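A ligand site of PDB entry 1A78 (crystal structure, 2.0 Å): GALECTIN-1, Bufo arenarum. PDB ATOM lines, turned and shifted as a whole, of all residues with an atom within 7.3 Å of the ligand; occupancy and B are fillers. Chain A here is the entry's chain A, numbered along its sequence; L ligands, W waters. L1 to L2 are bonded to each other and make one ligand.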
ATOM      1  N   ALA A  32      12.501  -8.706  28.830  1.00  0.00           N
ATOM      2  CA  ALA A  32      12.787  -7.420  29.443  1.00  0.00           C
ATOM      3  C   ALA A  32      13.570  -7.542  30.741  1.00  0.00           C
ATOM      4  O   ALA A  32      13.589  -8.587  31.370  1.00  0.00           O
ATOM      5  CB  ALA A  32      11.480  -6.646  29.689  1.00  0.00           C
ATOM      6  N   HIS A  45      13.382   0.463  31.411  1.00  0.00           N
ATOM      7  CA  HIS A  45      12.695  -0.752  30.961  1.00  0.00           C
ATOM      8  C   HIS A  45      13.441  -1.077  29.650  1.00  0.00           C
ATOM      9  O   HIS A  45      13.345  -0.337  28.662  1.00  0.00           O
ATOM     10  CB  HIS A  45      11.205  -0.538  30.679  1.00  0.00           C
ATOM     11  CG  HIS A  45      10.560  -1.649  29.890  1.00  0.00           C
ATOM     12  ND1 HIS A  45      10.090  -2.818  30.476  1.00  0.00           N
ATOM     13  CD2 HIS A  45      10.275  -1.771  28.566  1.00  0.00           C
ATOM     14  CE1 HIS A  45       9.557  -3.598  29.550  1.00  0.00           C
ATOM     15  NE2 HIS A  45       9.658  -2.990  28.389  1.00  0.00           N
ATOM     16  N   PHE A  46      14.238  -2.154  29.701  1.00  0.00           N
ATOM     17  CA  PHE A  46      15.046  -2.629  28.593  1.00  0.00           C
ATOM     18  C   PHE A  46      14.317  -3.813  27.949  1.00  0.00           C
ATOM     19  O   PHE A  46      14.343  -4.910  28.472  1.00  0.00           O
ATOM     20  CB  PHE A  46      16.395  -3.066  29.173  1.00  0.00           C
ATOM     21  CG  PHE A  46      17.305  -3.701  28.193  1.00  0.00           C
ATOM     22  CD1 PHE A  46      17.241  -5.063  27.967  1.00  0.00           C
ATOM     23  CD2 PHE A  46      18.206  -2.941  27.481  1.00  0.00           C
ATOM     24  CE1 PHE A  46      18.056  -5.656  27.033  1.00  0.00           C
ATOM     25  CE2 PHE A  46      19.052  -3.523  26.544  1.00  0.00           C
ATOM     26  CZ  PHE A  46      18.975  -4.885  26.314  1.00  0.00           C
ATOM     27  N   ASN A  47      13.706  -3.598  26.798  1.00  0.00           N
ATOM     28  CA  ASN A  47      12.927  -4.654  26.154  1.00  0.00           C
ATOM     29  C   ASN A  47      13.501  -5.114  24.791  1.00  0.00           C
ATOM     30  O   ASN A  47      13.478  -4.349  23.816  1.00  0.00           O
ATOM     31  CB  ASN A  47      11.498  -4.131  26.013  1.00  0.00           C
ATOM     32  CG  ASN A  47      10.504  -5.174  25.525  1.00  0.00           C
ATOM     33  OD1 ASN A  47       9.382  -4.815  25.195  1.00  0.00           O
ATOM     34  ND2 ASN A  47      10.884  -6.458  25.522  1.00  0.00           N
ATOM     35  N   ARG A  49      12.986  -7.039  21.681  1.00  0.00           N
ATOM     36  CA  ARG A  49      11.875  -7.600  20.903  1.00  0.00           C
ATOM     37  C   ARG A  49      12.261  -8.435  19.694  1.00  0.00           C
ATOM     38  O   ARG A  49      12.669  -7.905  18.676  1.00  0.00           O
ATOM     39  CB  ARG A  49      10.942  -6.462  20.470  1.00  0.00           C
ATOM     40  CG  ARG A  49      10.365  -5.684  21.652  1.00  0.00           C
ATOM     41  CD  ARG A  49       9.414  -4.583  21.241  1.00  0.00           C
ATOM     42  NE  ARG A  49       8.787  -3.954  22.403  1.00  0.00           N
ATOM     43  CZ  ARG A  49       7.922  -2.949  22.356  1.00  0.00           C
ATOM     44  NH1 ARG A  49       7.528  -2.425  21.193  1.00  0.00           N
ATOM     45  NH2 ARG A  49       7.461  -2.430  23.479  1.00  0.00           N
ATOM     46  N   LEU A  52       7.708  -8.521  18.292  1.00  0.00           N
ATOM     47  CA  LEU A  52       6.667  -8.027  19.169  1.00  0.00           C
ATOM     48  C   LEU A  52       6.166  -6.617  18.814  1.00  0.00           C
ATOM     49  O   LEU A  52       6.940  -5.683  18.706  1.00  0.00           O
ATOM     50  CB  LEU A  52       7.174  -8.056  20.612  1.00  0.00           C
ATOM     51  CG  LEU A  52       6.194  -7.764  21.761  1.00  0.00           C
ATOM     52  CD1 LEU A  52       5.288  -8.982  21.959  1.00  0.00           C
ATOM     53  CD2 LEU A  52       6.991  -7.460  23.036  1.00  0.00           C
ATOM     54  N   HIS A  53       4.839  -6.483  18.663  1.00  0.00           N
ATOM     55  CA  HIS A  53       4.197  -5.201  18.336  1.00  0.00           C
ATOM     56  C   HIS A  53       4.728  -4.547  17.069  1.00  0.00           C
ATOM     57  O   HIS A  53       4.818  -3.319  17.017  1.00  0.00           O
ATOM     58  CB  HIS A  53       4.371  -4.184  19.457  1.00  0.00           C
ATOM     59  CG  HIS A  53       3.870  -4.667  20.775  1.00  0.00           C
ATOM     60  ND1 HIS A  53       2.781  -5.507  20.894  1.00  0.00           N
ATOM     61  CD2 HIS A  53       4.344  -4.477  22.022  1.00  0.00           C
ATOM     62  CE1 HIS A  53       2.613  -5.813  22.172  1.00  0.00           C
ATOM     63  NE2 HIS A  53       3.550  -5.211  22.873  1.00  0.00           N
ATOM     64  N   ASP A  55       7.739  -4.662  16.088  1.00  0.00           N
ATOM     65  CA  ASP A  55       9.194  -4.510  16.246  1.00  0.00           C
ATOM     66  C   ASP A  55       9.787  -5.918  16.077  1.00  0.00           C
ATOM     67  O   ASP A  55       9.410  -6.846  16.786  1.00  0.00           O
ATOM     68  CB  ASP A  55       9.534  -3.963  17.644  1.00  0.00           C
ATOM     69  CG  ASP A  55       9.280  -2.479  17.759  1.00  0.00           C
ATOM     70  OD1 ASP A  55       9.511  -1.754  16.778  1.00  0.00           O
ATOM     71  OD2 ASP A  55       8.888  -2.015  18.848  1.00  0.00           O
ATOM     72  N   VAL A  60      13.845  -1.877  22.592  1.00  0.00           N
ATOM     73  CA  VAL A  60      13.088  -0.680  22.957  1.00  0.00           C
ATOM     74  C   VAL A  60      13.399  -0.342  24.422  1.00  0.00           C
ATOM     75  O   VAL A  60      13.424  -1.237  25.243  1.00  0.00           O
ATOM     76  CB  VAL A  60      11.571  -0.906  22.773  1.00  0.00           C
ATOM     77  CG1 VAL A  60      10.803   0.341  23.149  1.00  0.00           C
ATOM     78  CG2 VAL A  60      11.278  -1.284  21.332  1.00  0.00           C
ATOM     79  N   CYS A  61      13.734   0.898  24.737  1.00  0.00           N
ATOM     80  CA  CYS A  61      14.028   1.275  26.116  1.00  0.00           C
ATOM     81  C   CYS A  61      13.081   2.382  26.490  1.00  0.00           C
ATOM     82  O   CYS A  61      12.754   3.224  25.649  1.00  0.00           O
ATOM     83  CB  CYS A  61      15.474   1.772  26.276  1.00  0.00           C
ATOM     84  SG  CYS A  61      16.726   0.501  26.149  1.00  0.00           S
ATOM     85  N   ASN A  62      12.637   2.392  27.735  1.00  0.00           N
ATOM     86  CA  ASN A  62      11.729   3.458  28.170  1.00  0.00           C
ATOM     87  C   ASN A  62      11.777   3.587  29.671  1.00  0.00           C
ATOM     88  O   ASN A  62      12.446   2.792  30.351  1.00  0.00           O
ATOM     89  CB  ASN A  62      10.294   3.165  27.722  1.00  0.00           C
ATOM     90  CG  ASN A  62       9.467   4.406  27.550  1.00  0.00           C
ATOM     91  OD1 ASN A  62       9.857   5.501  27.953  1.00  0.00           O
ATOM     92  ND2 ASN A  62       8.300   4.252  26.954  1.00  0.00           N
ATOM     93  N   SER A  63      11.170   4.655  30.195  1.00  0.00           N
ATOM     94  CA  SER A  63      11.099   4.873  31.627  1.00  0.00           C
ATOM     95  C   SER A  63       9.604   4.803  31.918  1.00  0.00           C
ATOM     96  O   SER A  63       8.793   4.911  31.006  1.00  0.00           O
ATOM     97  CB  SER A  63      11.634   6.243  32.001  1.00  0.00           C
ATOM     98  OG  SER A  63      10.841   7.254  31.418  1.00  0.00           O
ATOM     99  N   TRP A  69       4.127   5.168  30.777  1.00  0.00           N
ATOM    100  CA  TRP A  69       5.348   5.052  30.005  1.00  0.00           C
ATOM    101  C   TRP A  69       5.799   6.415  29.471  1.00  0.00           C
ATOM    102  O   TRP A  69       4.986   7.314  29.286  1.00  0.00           O
ATOM    103  CB  TRP A  69       5.130   4.107  28.862  1.00  0.00           C
ATOM    104  CG  TRP A  69       4.959   2.712  29.292  1.00  0.00           C
ATOM    105  CD1 TRP A  69       3.820   1.984  29.261  1.00  0.00           C
ATOM    106  CD2 TRP A  69       5.985   1.827  29.744  1.00  0.00           C
ATOM    107  NE1 TRP A  69       4.053   0.707  29.662  1.00  0.00           N
ATOM    108  CE2 TRP A  69       5.385   0.577  29.969  1.00  0.00           C
ATOM    109  CE3 TRP A  69       7.360   1.967  29.983  1.00  0.00           C
ATOM    110  CZ2 TRP A  69       6.100  -0.549  30.425  1.00  0.00           C
ATOM    111  CZ3 TRP A  69       8.079   0.855  30.429  1.00  0.00           C
ATOM    112  CH2 TRP A  69       7.439  -0.381  30.647  1.00  0.00           C
ATOM    113  N   GLY A  70       7.103   6.587  29.315  1.00  0.00           N
ATOM    114  CA  GLY A  70       7.660   7.853  28.807  1.00  0.00           C
ATOM    115  C   GLY A  70       8.026   7.741  27.332  1.00  0.00           C
ATOM    116  O   GLY A  70       7.468   6.906  26.620  1.00  0.00           O
ATOM    117  N   SER A  71       8.995   8.504  26.871  1.00  0.00           N
ATOM    118  CA  SER A  71       9.379   8.424  25.457  1.00  0.00           C
ATOM    119  C   SER A  71      10.273   7.258  25.142  1.00  0.00           C
ATOM    120  O   SER A  71      11.373   7.160  25.681  1.00  0.00           O
ATOM    121  CB  SER A  71      10.097   9.695  25.013  1.00  0.00           C
ATOM    122  OG  SER A  71       9.437  10.843  25.522  1.00  0.00           O
ATOM    123  N   GLU A  72       9.838   6.407  24.231  1.00  0.00           N
ATOM    124  CA  GLU A  72      10.635   5.240  23.865  1.00  0.00           C
ATOM    125  C   GLU A  72      11.905   5.693  23.146  1.00  0.00           C
ATOM    126  O   GLU A  72      11.923   6.764  22.528  1.00  0.00           O
ATOM    127  CB  GLU A  72       9.861   4.301  22.943  1.00  0.00           C
ATOM    128  CG  GLU A  72       8.589   3.679  23.533  1.00  0.00           C
ATOM    129  CD  GLU A  72       8.084   2.499  22.711  1.00  0.00           C
ATOM    130  OE1 GLU A  72       8.467   2.395  21.543  1.00  0.00           O
ATOM    131  OE2 GLU A  72       7.313   1.659  23.223  1.00  0.00           O
ATOM    132  N   GLN A  73      12.950   4.886  23.274  1.00  0.00           N
ATOM    133  CA  GLN A  73      14.227   5.109  22.619  1.00  0.00           C
ATOM    134  C   GLN A  73      14.490   3.748  22.007  1.00  0.00           C
ATOM    135  O   GLN A  73      14.670   2.780  22.737  1.00  0.00           O
ATOM    136  CB  GLN A  73      15.340   5.459  23.603  1.00  0.00           C
ATOM    137  CG  GLN A  73      16.749   5.340  22.985  1.00  0.00           C
ATOM    138  CD  GLN A  73      17.870   5.804  23.905  1.00  0.00           C
ATOM    139  OE1 GLN A  73      17.808   6.884  24.485  1.00  0.00           O
ATOM    140  NE2 GLN A  73      18.910   4.974  24.040  1.00  0.00           N
ATOM    141  N   ARG A  74      14.399   3.649  20.686  1.00  0.00           N
ATOM    142  CA  ARG A  74      14.645   2.372  20.040  1.00  0.00           C
ATOM    143  C   ARG A  74      16.117   2.240  19.659  1.00  0.00           C
ATOM    144  O   ARG A  74      16.814   3.246  19.597  1.00  0.00           O
ATOM    145  CB  ARG A  74      13.760   2.216  18.806  1.00  0.00           C
ATOM    146  CG  ARG A  74      12.311   1.925  19.128  1.00  0.00           C
ATOM    147  CD  ARG A  74      11.614   1.227  17.964  1.00  0.00           C
ATOM    148  NE  ARG A  74      10.318   0.647  18.353  1.00  0.00           N
ATOM    149  CZ  ARG A  74       9.342   1.320  18.949  1.00  0.00           C
ATOM    150  NH1 ARG A  74       9.491   2.615  19.211  1.00  0.00           N
ATOM    151  NH2 ARG A  74       8.253   0.690  19.369  1.00  0.00           N
ATOM    152  N   GLU A 124      11.580 -10.321  32.869  1.00  0.00           N
ATOM    153  CA  GLU A 124      10.336 -10.822  32.323  1.00  0.00           C
ATOM    154  C   GLU A 124      10.659 -11.713  31.132  1.00  0.00           C
ATOM    155  O   GLU A 124      11.347 -11.286  30.204  1.00  0.00           O
ATOM    156  CB  GLU A 124       9.445  -9.681  31.842  1.00  0.00           C
ATOM    157  CG  GLU A 124       9.139  -8.549  32.825  1.00  0.00           C
ATOM    158  CD  GLU A 124       8.401  -7.399  32.124  1.00  0.00           C
ATOM    159  OE1 GLU A 124       7.958  -7.593  30.954  1.00  0.00           O
ATOM    160  OE2 GLU A 124       8.268  -6.286  32.708  1.00  0.00           O
HETATM  161  C1  LIG L   1       4.630  -1.056  25.273  1.00  0.00           C
HETATM  162  C2  LIG L   1       4.817  -2.412  25.904  1.00  0.00           C
HETATM  163  C3  LIG L   1       5.454  -2.257  27.273  1.00  0.00           C
HETATM  164  C4  LIG L   1       6.787  -1.587  27.097  1.00  0.00           C
HETATM  165  C5  LIG L   1       6.587  -0.240  26.398  1.00  0.00           C
HETATM  166  C6  LIG L   1       7.893   0.445  26.074  1.00  0.00           C
HETATM  167  O1  LIG L   1       3.567  -3.049  26.030  1.00  0.00           O
HETATM  168  O2  LIG L   1       5.652  -3.541  27.837  1.00  0.00           O
HETATM  169  O3  LIG L   1       7.632  -2.431  26.327  1.00  0.00           O
HETATM  170  O4  LIG L   1       5.885  -0.387  25.144  1.00  0.00           O
HETATM  171  O5  LIG L   1       7.657   1.823  25.818  1.00  0.00           O
HETATM  172  S1  LIG L   1       4.148  -1.403  23.556  1.00  0.00           S
HETATM  173  C1  LG2 L   2       4.003   0.318  22.961  1.00  0.00           C
HETATM  174  C2  LG2 L   2       4.727   0.455  21.613  1.00  0.00           C
HETATM  175  C3  LG2 L   2       4.709   1.911  21.145  1.00  0.00           C
HETATM  176  C4  LG2 L   2       3.273   2.441  21.119  1.00  0.00           C
HETATM  177  C5  LG2 L   2       2.662   2.269  22.498  1.00  0.00           C
HETATM  178  C6  LG2 L   2       1.230   2.741  22.486  1.00  0.00           C
HETATM  179  O1  LG2 L   2       6.061   0.005  21.702  1.00  0.00           O
HETATM  180  O2  LG2 L   2       5.283   1.998  19.845  1.00  0.00           O
HETATM  181  O3  LG2 L   2       2.490   1.705  20.186  1.00  0.00           O
HETATM  182  O4  LG2 L   2       2.671   0.858  22.854  1.00  0.00           O
HETATM  183  O5  LG2 L   2       0.541   2.287  23.635  1.00  0.00           O
HETATM  184  O   HOH W   1       5.274   2.711  25.444  1.00  0.00           O
HETATM  185  O   HOH W   2       7.479  -5.369  27.100  1.00  0.00           O
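OE2 of Glu 72 is in hydrogen-bond range of O1 of LG2 L2. ND2 of Asn 62 is in hydrogen-bond range of O5 of LIG L1 (2.8 Å). O3 of LIG L1 lies within hydrogen-bond range of NH2 of Arg 49 (2.9 Å). NE2 of His 45 sits at hydrogen-bond distance from O3 of LIG L1. OD1 of Asn 47 sits at hydrogen-bond distance from O3 of LIG L1, at 3.2 Å. NH2 of Arg 74 sits at hydrogen-bond distance from O1 of LG2 L2.
The side-chain carboxylate of Glu 72 is in salt-bridge range of the guanidinium group of Arg 74 (2.6 Å). N of His 45 is in hydrogen-bond range of O of Asn 62 (2.7 Å). The side-chain amide nitrogen of Asn 62 sits at hydrogen-bond distance from the backbone carbonyl oxygen of Gly 70 (2.8 Å). The side-chain amide oxygen (OD1) of Asn 62 lies close to the backbone carbonyl oxygen (O) of Ser 71, 3.2 Å away. The side-chain amide oxygen (OD1) of Asn 47 lies within hydrogen-bond range of the guanidinium group (NE) of Arg 49 (3.0 Å). The guanidinium group of Arg 49 lies within salt-bridge range of the side-chain carboxylate of Asp 55 (2.7 Å). O of Asn 47 is in hydrogen-bond range of N of Val 60, at 2.8 Å. NH2 of Arg 74 is in salt-bridge range of OD2 of Asp 55, at 2.8 Å.
Residues that only touch the ligand: His 53 and Trp 69. Hydrophobic or aromatic side chains that line the ligand: His 45, His 53 and Trp 69. Within 4 Å of the ligand: His 45, Asn 47, Arg 49, His 53, Asn 62, Trp 69, Glu 72 and Arg 74.
Water W1 lies within hydrogen-bond range of an oxygen (O5) of LIG L1 and the side-chain carboxylate of Glu 72. Water W2 lies within hydrogen-bond range of an oxygen (O2) of LIG L1 (2.7 Å), the side-chain amide oxygen of Asn 47 (2.7 Å) and a ring nitrogen (NE2) of His 45 (3.5 Å).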
